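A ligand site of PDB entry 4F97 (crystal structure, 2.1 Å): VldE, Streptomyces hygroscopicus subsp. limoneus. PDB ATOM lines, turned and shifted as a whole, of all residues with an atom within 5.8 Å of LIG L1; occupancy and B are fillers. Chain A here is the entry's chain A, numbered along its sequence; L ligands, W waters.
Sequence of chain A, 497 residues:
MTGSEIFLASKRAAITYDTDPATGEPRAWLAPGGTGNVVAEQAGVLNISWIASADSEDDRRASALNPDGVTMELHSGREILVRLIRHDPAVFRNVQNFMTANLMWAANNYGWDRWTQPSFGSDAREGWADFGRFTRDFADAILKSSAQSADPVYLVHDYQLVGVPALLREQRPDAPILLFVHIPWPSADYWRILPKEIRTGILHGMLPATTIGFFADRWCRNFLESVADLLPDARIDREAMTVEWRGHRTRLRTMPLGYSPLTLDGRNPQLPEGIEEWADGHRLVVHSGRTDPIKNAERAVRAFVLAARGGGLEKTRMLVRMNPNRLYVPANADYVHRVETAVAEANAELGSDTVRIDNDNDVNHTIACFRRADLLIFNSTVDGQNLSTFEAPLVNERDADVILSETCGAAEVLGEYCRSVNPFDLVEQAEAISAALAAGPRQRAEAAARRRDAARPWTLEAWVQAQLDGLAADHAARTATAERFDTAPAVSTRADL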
ATOM      1  N   TRP A 105      10.280  10.503   6.086  1.00  0.00           N
ATOM      2  CA  TRP A 105       9.872  10.239   4.688  1.00  0.00           C
ATOM      3  C   TRP A 105       9.619  11.555   3.934  1.00  0.00           C
ATOM      4  O   TRP A 105      10.073  11.715   2.822  1.00  0.00           O
ATOM      5  CB  TRP A 105       8.604   9.387   4.628  1.00  0.00           C
ATOM      6  CG  TRP A 105       8.307   8.859   3.243  1.00  0.00           C
ATOM      7  CD1 TRP A 105       7.348   9.288   2.403  1.00  0.00           C
ATOM      8  CD2 TRP A 105       9.012   7.833   2.558  1.00  0.00           C
ATOM      9  NE1 TRP A 105       7.363   8.569   1.235  1.00  0.00           N
ATOM     10  CE2 TRP A 105       8.387   7.651   1.314  1.00  0.00           C
ATOM     11  CE3 TRP A 105      10.096   7.007   2.895  1.00  0.00           C
ATOM     12  CZ2 TRP A 105       8.823   6.703   0.389  1.00  0.00           C
ATOM     13  CZ3 TRP A 105      10.504   6.037   1.982  1.00  0.00           C
ATOM     14  CH2 TRP A 105       9.893   5.926   0.744  1.00  0.00           C
ATOM     15  N   THR A 263      11.557 -12.409 -10.161  1.00  0.00           N
ATOM     16  CA  THR A 263      10.225 -11.868 -10.432  1.00  0.00           C
ATOM     17  C   THR A 263       9.605 -12.491 -11.697  1.00  0.00           C
ATOM     18  O   THR A 263       9.847 -12.041 -12.810  1.00  0.00           O
ATOM     19  CB  THR A 263      10.259 -10.333 -10.552  1.00  0.00           C
ATOM     20  OG1 THR A 263      10.965  -9.945 -11.749  1.00  0.00           O
ATOM     21  CG2 THR A 263      10.929  -9.713  -9.333  1.00  0.00           C
ATOM     22  N   SER A 288       1.200   1.728 -11.351  1.00  0.00           N
ATOM     23  CA  SER A 288       1.286   0.898 -10.177  1.00  0.00           C
ATOM     24  C   SER A 288       2.225   1.502  -9.150  1.00  0.00           C
ATOM     25  O   SER A 288       3.296   1.957  -9.520  1.00  0.00           O
ATOM     26  CB  SER A 288       1.817  -0.498 -10.549  1.00  0.00           C
ATOM     27  OG  SER A 288       2.064  -1.255  -9.395  1.00  0.00           O
ATOM     28  N   ARG A 290       2.771   1.623  -4.416  1.00  0.00           N
ATOM     29  CA  ARG A 290       2.219   1.691  -3.073  1.00  0.00           C
ATOM     30  C   ARG A 290       1.345   2.950  -2.888  1.00  0.00           C
ATOM     31  O   ARG A 290       1.450   3.906  -3.667  1.00  0.00           O
ATOM     32  CB  ARG A 290       3.344   1.777  -2.040  1.00  0.00           C
ATOM     33  CG  ARG A 290       4.116   0.515  -1.749  1.00  0.00           C
ATOM     34  CD  ARG A 290       5.189   0.766  -0.655  1.00  0.00           C
ATOM     35  NE  ARG A 290       6.221   1.712  -1.098  1.00  0.00           N
ATOM     36  CZ  ARG A 290       6.350   2.983  -0.686  1.00  0.00           C
ATOM     37  NH1 ARG A 290       5.549   3.500   0.229  1.00  0.00           N
ATOM     38  NH2 ARG A 290       7.311   3.743  -1.186  1.00  0.00           N
ATOM     39  N   ILE A 294       4.322   9.913  -3.124  1.00  0.00           N
ATOM     40  CA  ILE A 294       5.349  10.046  -4.178  1.00  0.00           C
ATOM     41  C   ILE A 294       4.989   9.290  -5.464  1.00  0.00           C
ATOM     42  O   ILE A 294       5.591   9.538  -6.492  1.00  0.00           O
ATOM     43  CB  ILE A 294       6.739   9.536  -3.731  1.00  0.00           C
ATOM     44  CG1 ILE A 294       6.738   8.015  -3.562  1.00  0.00           C
ATOM     45  CG2 ILE A 294       7.227  10.243  -2.503  1.00  0.00           C
ATOM     46  CD1 ILE A 294       8.096   7.446  -3.231  1.00  0.00           C
ATOM     47  N   LYS A 295       4.070   8.323  -5.411  1.00  0.00           N
ATOM     48  CA  LYS A 295       3.833   7.483  -6.581  1.00  0.00           C
ATOM     49  C   LYS A 295       3.028   8.239  -7.612  1.00  0.00           C
ATOM     50  O   LYS A 295       3.011   7.822  -8.770  1.00  0.00           O
ATOM     51  CB  LYS A 295       3.096   6.205  -6.204  1.00  0.00           C
ATOM     52  CG  LYS A 295       3.844   5.290  -5.258  1.00  0.00           C
ATOM     53  CD  LYS A 295       5.198   4.873  -5.848  1.00  0.00           C
ATOM     54  CE  LYS A 295       6.171   4.460  -4.760  1.00  0.00           C
ATOM     55  NZ  LYS A 295       7.515   4.109  -5.243  1.00  0.00           N
ATOM     56  N   ARG A 321      -3.232   0.551 -10.010  1.00  0.00           N
ATOM     57  CA  ARG A 321      -2.943  -0.593  -9.173  1.00  0.00           C
ATOM     58  C   ARG A 321      -2.170  -0.068  -7.986  1.00  0.00           C
ATOM     59  O   ARG A 321      -1.142   0.542  -8.182  1.00  0.00           O
ATOM     60  CB  ARG A 321      -2.075  -1.569  -9.950  1.00  0.00           C
ATOM     61  CG  ARG A 321      -1.489  -2.676  -9.125  1.00  0.00           C
ATOM     62  CD  ARG A 321      -2.472  -3.804  -8.833  1.00  0.00           C
ATOM     63  NE  ARG A 321      -1.836  -4.818  -7.984  1.00  0.00           N
ATOM     64  CZ  ARG A 321      -2.477  -5.543  -7.063  1.00  0.00           C
ATOM     65  NH1 ARG A 321      -3.776  -5.381  -6.862  1.00  0.00           N
ATOM     66  NH2 ARG A 321      -1.826  -6.414  -6.326  1.00  0.00           N
ATOM     67  N   MET A 322      -2.689  -0.250  -6.767  1.00  0.00           N
ATOM     68  CA  MET A 322      -2.000   0.241  -5.579  1.00  0.00           C
ATOM     69  C   MET A 322      -1.804  -0.894  -4.586  1.00  0.00           C
ATOM     70  O   MET A 322      -2.571  -1.830  -4.510  1.00  0.00           O
ATOM     71  CB  MET A 322      -2.757   1.401  -4.906  1.00  0.00           C
ATOM     72  CG  MET A 322      -3.424   2.364  -5.827  1.00  0.00           C
ATOM     73  SD  MET A 322      -4.020   3.874  -5.008  1.00  0.00           S
ATOM     74  CE  MET A 322      -2.478   4.588  -4.566  1.00  0.00           C
ATOM     75  N   ASN A 323      -0.741  -0.802  -3.826  1.00  0.00           N
ATOM     76  CA  ASN A 323      -0.473  -1.794  -2.810  1.00  0.00           C
ATOM     77  C   ASN A 323      -0.569  -1.048  -1.484  1.00  0.00           C
ATOM     78  O   ASN A 323       0.218  -0.145  -1.211  1.00  0.00           O
ATOM     79  CB  ASN A 323       0.912  -2.437  -3.034  1.00  0.00           C
ATOM     80  CG  ASN A 323       1.378  -3.238  -1.831  1.00  0.00           C
ATOM     81  OD1 ASN A 323       0.554  -3.662  -1.001  1.00  0.00           O
ATOM     82  ND2 ASN A 323       2.698  -3.434  -1.715  1.00  0.00           N
ATOM     83  N   ASP A 360      -4.740  -3.583  -3.482  1.00  0.00           N
ATOM     84  CA  ASP A 360      -4.640  -4.845  -2.759  1.00  0.00           C
ATOM     85  C   ASP A 360      -3.168  -5.234  -2.716  1.00  0.00           C
ATOM     86  O   ASP A 360      -2.415  -4.911  -3.611  1.00  0.00           O
ATOM     87  CB  ASP A 360      -5.541  -5.917  -3.449  1.00  0.00           C
ATOM     88  CG  ASP A 360      -5.221  -7.363  -3.051  1.00  0.00           C
ATOM     89  OD1 ASP A 360      -6.015  -8.258  -3.428  1.00  0.00           O
ATOM     90  OD2 ASP A 360      -4.163  -7.595  -2.437  1.00  0.00           O
ATOM     91  N   ASN A 361      -2.772  -5.935  -1.671  1.00  0.00           N
ATOM     92  CA  ASN A 361      -1.413  -6.410  -1.538  1.00  0.00           C
ATOM     93  C   ASN A 361      -1.227  -7.831  -2.118  1.00  0.00           C
ATOM     94  O   ASN A 361      -1.293  -8.832  -1.383  1.00  0.00           O
ATOM     95  CB  ASN A 361      -1.010  -6.373  -0.065  1.00  0.00           C
ATOM     96  CG  ASN A 361       0.326  -6.981   0.185  1.00  0.00           C
ATOM     97  OD1 ASN A 361       1.053  -7.299  -0.750  1.00  0.00           O
ATOM     98  ND2 ASN A 361       0.669  -7.153   1.452  1.00  0.00           N
ATOM     99  N   ASP A 362      -1.011  -7.936  -3.439  1.00  0.00           N
ATOM    100  CA  ASP A 362      -0.738  -9.223  -4.088  1.00  0.00           C
ATOM    101  C   ASP A 362       0.225  -9.028  -5.235  1.00  0.00           C
ATOM    102  O   ASP A 362      -0.174  -8.707  -6.337  1.00  0.00           O
ATOM    103  CB  ASP A 362      -2.008  -9.880  -4.605  1.00  0.00           C
ATOM    104  CG  ASP A 362      -1.783 -11.325  -5.072  1.00  0.00           C
ATOM    105  OD1 ASP A 362      -0.696 -11.653  -5.589  1.00  0.00           O
ATOM    106  OD2 ASP A 362      -2.720 -12.134  -4.904  1.00  0.00           O
ATOM    107  N   VAL A 363       1.513  -9.211  -4.967  1.00  0.00           N
ATOM    108  CA  VAL A 363       2.546  -8.947  -5.931  1.00  0.00           C
ATOM    109  C   VAL A 363       2.299  -9.691  -7.264  1.00  0.00           C
ATOM    110  O   VAL A 363       2.578  -9.153  -8.327  1.00  0.00           O
ATOM    111  CB  VAL A 363       3.958  -9.247  -5.343  1.00  0.00           C
ATOM    112  CG1 VAL A 363       4.181 -10.743  -5.191  1.00  0.00           C
ATOM    113  CG2 VAL A 363       5.068  -8.633  -6.245  1.00  0.00           C
ATOM    114  N   THR A 366       0.113  -7.808  -9.423  1.00  0.00           N
ATOM    115  CA  THR A 366       0.710  -6.617 -10.047  1.00  0.00           C
ATOM    116  C   THR A 366       1.530  -7.029 -11.248  1.00  0.00           C
ATOM    117  O   THR A 366       1.434  -6.431 -12.326  1.00  0.00           O
ATOM    118  CB  THR A 366       1.568  -5.793  -9.074  1.00  0.00           C
ATOM    119  OG1 THR A 366       0.727  -5.359  -7.989  1.00  0.00           O
ATOM    120  CG2 THR A 366       2.140  -4.575  -9.791  1.00  0.00           C
ATOM    121  N   ILE A 367       2.313  -8.080 -11.091  1.00  0.00           N
ATOM    122  CA  ILE A 367       3.032  -8.611 -12.237  1.00  0.00           C
ATOM    123  C   ILE A 367       2.084  -8.950 -13.399  1.00  0.00           C
ATOM    124  O   ILE A 367       2.411  -8.690 -14.567  1.00  0.00           O
ATOM    125  CB  ILE A 367       3.922  -9.835 -11.857  1.00  0.00           C
ATOM    126  CG1 ILE A 367       4.818  -9.481 -10.656  1.00  0.00           C
ATOM    127  CG2 ILE A 367       4.707 -10.304 -13.066  1.00  0.00           C
ATOM    128  CD1 ILE A 367       5.917  -8.482 -10.971  1.00  0.00           C
ATOM    129  N   PHE A 370       1.364  -5.842 -15.174  1.00  0.00           N
ATOM    130  CA  PHE A 370       2.523  -5.433 -15.988  1.00  0.00           C
ATOM    131  C   PHE A 370       2.535  -6.127 -17.363  1.00  0.00           C
ATOM    132  O   PHE A 370       2.740  -5.486 -18.399  1.00  0.00           O
ATOM    133  CB  PHE A 370       3.853  -5.736 -15.240  1.00  0.00           C
ATOM    134  CG  PHE A 370       4.144  -4.828 -14.032  1.00  0.00           C
ATOM    135  CD1 PHE A 370       3.370  -3.693 -13.769  1.00  0.00           C
ATOM    136  CD2 PHE A 370       5.211  -5.102 -13.186  1.00  0.00           C
ATOM    137  CE1 PHE A 370       3.661  -2.860 -12.669  1.00  0.00           C
ATOM    138  CE2 PHE A 370       5.488  -4.308 -12.093  1.00  0.00           C
ATOM    139  CZ  PHE A 370       4.715  -3.172 -11.831  1.00  0.00           C
ATOM    140  N   ASP A 383      11.541   9.265  -6.631  1.00  0.00           N
ATOM    141  CA  ASP A 383      11.739   7.903  -6.155  1.00  0.00           C
ATOM    142  C   ASP A 383      13.214   7.607  -5.915  1.00  0.00           C
ATOM    143  O   ASP A 383      14.076   8.106  -6.648  1.00  0.00           O
ATOM    144  CB  ASP A 383      11.142   6.892  -7.143  1.00  0.00           C
ATOM    145  CG  ASP A 383      10.127   5.970  -6.483  1.00  0.00           C
ATOM    146  OD1 ASP A 383      10.377   5.529  -5.345  1.00  0.00           O
ATOM    147  OD2 ASP A 383       9.094   5.695  -7.111  1.00  0.00           O
ATOM    148  N   GLN A 385      14.716   4.800  -6.402  1.00  0.00           N
ATOM    149  CA  GLN A 385      15.079   4.190  -7.671  1.00  0.00           C
ATOM    150  C   GLN A 385      13.820   3.913  -8.488  1.00  0.00           C
ATOM    151  O   GLN A 385      13.617   4.481  -9.537  1.00  0.00           O
ATOM    152  CB  GLN A 385      15.848   2.899  -7.430  1.00  0.00           C
ATOM    153  CG  GLN A 385      16.315   2.182  -8.725  1.00  0.00           C
ATOM    154  CD  GLN A 385      17.422   2.948  -9.455  1.00  0.00           C
ATOM    155  OE1 GLN A 385      17.679   4.148  -9.215  1.00  0.00           O
ATOM    156  NE2 GLN A 385      18.093   2.247 -10.337  1.00  0.00           N
ATOM    157  N   ASN A 386      13.011   3.014  -7.950  1.00  0.00           N
ATOM    158  CA  ASN A 386      11.824   2.508  -8.595  1.00  0.00           C
ATOM    159  C   ASN A 386      12.236   1.288  -9.389  1.00  0.00           C
ATOM    160  O   ASN A 386      12.716   1.387 -10.515  1.00  0.00           O
ATOM    161  CB  ASN A 386      11.164   3.548  -9.495  1.00  0.00           C
ATOM    162  CG  ASN A 386       9.762   3.135  -9.907  1.00  0.00           C
ATOM    163  OD1 ASN A 386       9.566   2.109 -10.552  1.00  0.00           O
ATOM    164  ND2 ASN A 386       8.777   3.934  -9.516  1.00  0.00           N
ATOM    165  N   LEU A 387      12.039   0.127  -8.785  1.00  0.00           N
ATOM    166  CA  LEU A 387      12.329  -1.157  -9.449  1.00  0.00           C
ATOM    167  C   LEU A 387      11.214  -1.563 -10.416  1.00  0.00           C
ATOM    168  O   LEU A 387      11.421  -2.350 -11.320  1.00  0.00           O
ATOM    169  CB  LEU A 387      12.511  -2.266  -8.434  1.00  0.00           C
ATOM    170  CG  LEU A 387      13.470  -2.025  -7.260  1.00  0.00           C
ATOM    171  CD1 LEU A 387      13.759  -3.328  -6.448  1.00  0.00           C
ATOM    172  CD2 LEU A 387      14.752  -1.359  -7.752  1.00  0.00           C
ATOM    173  N   SER A 388      10.004  -1.043 -10.187  1.00  0.00           N
ATOM    174  CA  SER A 388       8.860  -1.459 -10.989  1.00  0.00           C
ATOM    175  C   SER A 388       9.105  -1.118 -12.434  1.00  0.00           C
ATOM    176  O   SER A 388       8.752  -1.871 -13.345  1.00  0.00           O
ATOM    177  CB  SER A 388       7.567  -0.814 -10.498  1.00  0.00           C
ATOM    178  OG  SER A 388       7.213  -1.246  -9.180  1.00  0.00           O
ATOM    179  N   THR A 389       9.731   0.029 -12.670  1.00  0.00           N
ATOM    180  CA  THR A 389       9.941   0.496 -14.026  1.00  0.00           C
ATOM    181  C   THR A 389      10.940  -0.373 -14.785  1.00  0.00           C
ATOM    182  O   THR A 389      11.019  -0.260 -16.017  1.00  0.00           O
ATOM    183  CB  THR A 389      10.383   1.999 -14.090  1.00  0.00           C
ATOM    184  OG1 THR A 389      10.325   2.437 -15.439  1.00  0.00           O
ATOM    185  CG2 THR A 389      11.811   2.170 -13.637  1.00  0.00           C
ATOM    186  N   GLU A 391      11.152  -3.931 -13.793  1.00  0.00           N
ATOM    187  CA  GLU A 391      10.391  -5.171 -13.860  1.00  0.00           C
ATOM    188  C   GLU A 391       9.324  -5.195 -14.954  1.00  0.00           C
ATOM    189  O   GLU A 391       9.110  -6.231 -15.629  1.00  0.00           O
ATOM    190  CB  GLU A 391       9.708  -5.456 -12.511  1.00  0.00           C
ATOM    191  CG  GLU A 391      10.638  -5.661 -11.330  1.00  0.00           C
ATOM    192  CD  GLU A 391       9.866  -5.569  -9.998  1.00  0.00           C
ATOM    193  OE1 GLU A 391       8.688  -5.160 -10.025  1.00  0.00           O
ATOM    194  OE2 GLU A 391      10.432  -5.919  -8.926  1.00  0.00           O
HETATM  195  P1  LIG L   1       8.927   1.159  -3.526  1.00  0.00           P
HETATM  196  O1  LIG L   1       7.572   0.704  -3.093  1.00  0.00           O
HETATM  197  O2  LIG L   1       9.017   2.676  -3.205  1.00  0.00           O
HETATM  198  O3  LIG L   1      10.149   0.551  -2.925  1.00  0.00           O
HETATM  199  O4  LIG L   1       8.911   1.102  -5.138  1.00  0.00           O
HETATM  200  P2  LIG L   1       9.635   0.096  -6.143  1.00  0.00           P
HETATM  201  O5  LIG L   1       8.938   0.327  -7.463  1.00  0.00           O
HETATM  202  O6  LIG L   1      11.133   0.178  -6.239  1.00  0.00           O
HETATM  203  O7  LIG L   1       9.271  -1.335  -5.478  1.00  0.00           O
HETATM  204  C1  LIG L   1       8.019  -1.938  -5.620  1.00  0.00           C
HETATM  205  C2  LIG L   1       8.232  -3.444  -5.426  1.00  0.00           C
HETATM  206  O8  LIG L   1       7.068  -4.061  -4.885  1.00  0.00           O
HETATM  207  C3  LIG L   1       8.451  -4.117  -6.762  1.00  0.00           C
HETATM  208  O9  LIG L   1       9.380  -5.182  -6.562  1.00  0.00           O
HETATM  209  C4  LIG L   1       7.071  -4.586  -7.164  1.00  0.00           C
HETATM  210  O10 LIG L   1       7.050  -5.649  -8.122  1.00  0.00           O
HETATM  211  C5  LIG L   1       6.520  -4.999  -5.811  1.00  0.00           C
HETATM  212  N1  LIG L   1       5.034  -5.030  -5.832  1.00  0.00           N
HETATM  213  C6  LIG L   1       4.214  -4.629  -6.812  1.00  0.00           C
HETATM  214  N2  LIG L   1       2.927  -4.842  -6.455  1.00  0.00           N
HETATM  215  C7  LIG L   1       2.911  -5.377  -5.223  1.00  0.00           C
HETATM  216  C8  LIG L   1       1.895  -5.831  -4.254  1.00  0.00           C
HETATM  217  O11 LIG L   1       0.669  -5.750  -4.514  1.00  0.00           O
HETATM  218  N3  LIG L   1       2.303  -6.268  -3.071  1.00  0.00           N
HETATM  219  C9  LIG L   1       3.599  -6.374  -2.740  1.00  0.00           C
HETATM  220  N4  LIG L   1       3.960  -6.876  -1.530  1.00  0.00           N
HETATM  221  N5  LIG L   1       4.592  -5.991  -3.593  1.00  0.00           N
HETATM  222  C10 LIG L   1       4.302  -5.483  -4.809  1.00  0.00           C
HETATM  223  O1  LG2 L   2       5.828   0.655   4.449  1.00  0.00           O
HETATM  224  P1  LG2 L   2       7.210   0.101   4.208  1.00  0.00           P
HETATM  225  O2  LG2 L   2       8.223   0.515   5.258  1.00  0.00           O
HETATM  226  O3  LG2 L   2       7.245  -1.353   3.841  1.00  0.00           O
HETATM  227  O4  LG2 L   2       7.710   0.847   2.869  1.00  0.00           O
HETATM  228  C1  LG2 L   2       8.093   0.097   1.725  1.00  0.00           C
HETATM  229  C2  LG2 L   2       9.521   0.460   1.343  1.00  0.00           C
HETATM  230  C3  LG2 L   2       9.521   1.790   0.603  1.00  0.00           C
HETATM  231  C4  LG2 L   2      10.408   0.505   2.575  1.00  0.00           C
HETATM  232  O5  LG2 L   2      10.454  -0.791   3.173  1.00  0.00           O
HETATM  233  C5  LG2 L   2      11.814   0.936   2.218  1.00  0.00           C
HETATM  234  O6  LG2 L   2      12.598   1.011   3.411  1.00  0.00           O
HETATM  235  C6  LG2 L   2      11.809   2.303   1.534  1.00  0.00           C
HETATM  236  O7  LG2 L   2      13.140   2.668   1.177  1.00  0.00           O
HETATM  237  C7  LG2 L   2      10.918   2.305   0.284  1.00  0.00           C
HETATM  238  N1  LG2 L   2      11.520   1.552  -0.810  1.00  0.00           N
HETATM  239  C8  LG2 L   2      12.746   2.025  -1.419  1.00  0.00           C
HETATM  240  C9  LG2 L   2      13.530   0.878  -2.031  1.00  0.00           C
HETATM  241  C10 LG2 L   2      12.492   3.184  -2.400  1.00  0.00           C
HETATM  242  O8  LG2 L   2      11.247   3.817  -2.076  1.00  0.00           O
HETATM  243  C11 LG2 L   2      12.444   2.780  -3.869  1.00  0.00           C
HETATM  244  O9  LG2 L   2      12.402   3.954  -4.675  1.00  0.00           O
HETATM  245  C12 LG2 L   2      13.676   1.968  -4.263  1.00  0.00           C
HETATM  246  O10 LG2 L   2      13.487   1.468  -5.593  1.00  0.00           O
HETATM  247  C13 LG2 L   2      13.890   0.824  -3.320  1.00  0.00           C
HETATM  248  C14 LG2 L   2      14.548  -0.438  -3.847  1.00  0.00           C
HETATM  249  O11 LG2 L   2      15.140  -1.167  -2.764  1.00  0.00           O
HETATM  250  O   HOH W   1       6.735   1.878  -7.203  1.00  0.00           O
HETATM  251  O   HOH W   2      -0.300  -3.469  -5.478  1.00  0.00           O
HETATM  252  O   HOH W   3       5.479   0.929  -4.718  1.00  0.00           O
HETATM  253  O   HOH W   4       7.173  -1.966  -1.749  1.00  0.00           O
HETATM  254  O   HOH W   5      11.242  -2.093  -3.215  1.00  0.00           O
HETATM  255  O   HOH W   6       4.968  -2.433  -3.310  1.00  0.00           O
HETATM  256  O   HOH W   7       4.013  -1.498  -5.699  1.00  0.00           O
HETATM  257  O   HOH W   8       4.563  -1.575  -8.375  1.00  0.00           O
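An oxygen (O3) of LIG L1 is in hydrogen-bond range of a nitrogen (N1) of LG2 L2.
Water W3 lies within hydrogen-bond range of O1 of LIG L1 (2.7 Å) and N of Arg 290 (2.8 Å).
Water W1 lies within hydrogen-bond range of O5 of LIG L1 and NZ of Lys 295.
Water W6 lies within hydrogen-bond range of ND2 of Asn 323 (2.9 Å) and O8 of LIG L1 (3.1 Å).
Water W8 bridges the side-chain hydroxyl of Ser 288 (2.7 Å) and the side-chain hydroxyl of Ser 388 (2.8 Å).
O11 of LIG L1 lies close to O of Asp 360.
N of Val 363 touches C8 of LIG L1 (3.5 Å).
OD1 of Asp 383 touches O2 of LIG L1, at 3.8 Å.
Asn 386 touches LIG L1 (CA to O6, 3.4 Å).
Hydrophobic or aromatic side chains within 4 Å of LIG L1: Val 363 and Leu 387.
The nearest printed residue that does not touch LIG L1 is Ile 367 (4.2 Å).
A nitrogen (N3) of LIG L1 sits close to the side-chain amide nitrogen of Asn 323 (3.2 Å).
NZ of Lys 295 is in salt-bridge range of O2 of LIG L1, 2.9 Å away.
O1 of LIG L1 lies within salt-bridge range of NE of Arg 290 (2.6 Å).
An oxygen (O6) of LIG L1 is in hydrogen-bond range of the backbone NH (N) of Leu 387 (2.7 Å).
O10 of LIG L1 sits at hydrogen-bond distance from OE1 of Glu 391, at 2.6 Å.
The side-chain carboxylate (OD1) of Asp 383 sits at hydrogen-bond distance from an oxygen (O9) of LG2 L2 (2.7 Å).
An oxygen (O5) of LIG L1 lies within hydrogen-bond range of the side-chain hydroxyl of Ser 388.
The guanidinium group (NH2) of Arg 321 is in hydrogen-bond range of an oxygen (O11) of LIG L1 (3.2 Å).
The backbone NH (N) of Gln 385 lies within hydrogen-bond range of an oxygen (O9) of LG2 L2.
OG1 of Thr 366 lies within hydrogen-bond range of N2 of LIG L1, at 2.7 Å.
The backbone NH of Asn 386 is in hydrogen-bond range of an oxygen (O10) of LG2 L2 (2.9 Å).
N of Ser 388 sits at hydrogen-bond distance from O5 of LIG L1 (3.2 Å).
A nitrogen (N3) of LIG L1 is in hydrogen-bond range of the side-chain amide oxygen (OD1) of Asn 361.
The backbone NH of Asp 362 lies within hydrogen-bond range of an oxygen (O11) of LIG L1, 3.0 Å away.
The guanidinium group of Arg 321 is in hydrogen-bond range of the backbone carbonyl oxygen of Asp 360 (3.2 Å).
The side-chain amide oxygen of Asn 386 sits at hydrogen-bond distance from the backbone NH of Thr 389.
The side-chain amino group of Lys 295 lies within salt-bridge range of the side-chain carboxylate of Asp 383 (2.9 Å).
The side-chain carboxylate (OD2) of Asp 383 is in hydrogen-bond range of the side-chain amide nitrogen (ND2) of Asn 386, at 3.0 Å.
NE of Arg 321 sits at hydrogen-bond distance from OG1 of Thr 366.
N of Asp 362 is in hydrogen-bond range of OD2 of Asp 360.
N of Asp 360 is in hydrogen-bond range of O of Met 322.
The side-chain amide oxygen of Asn 386 lies within hydrogen-bond range of the backbone NH of Ser 388 (3.2 Å).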
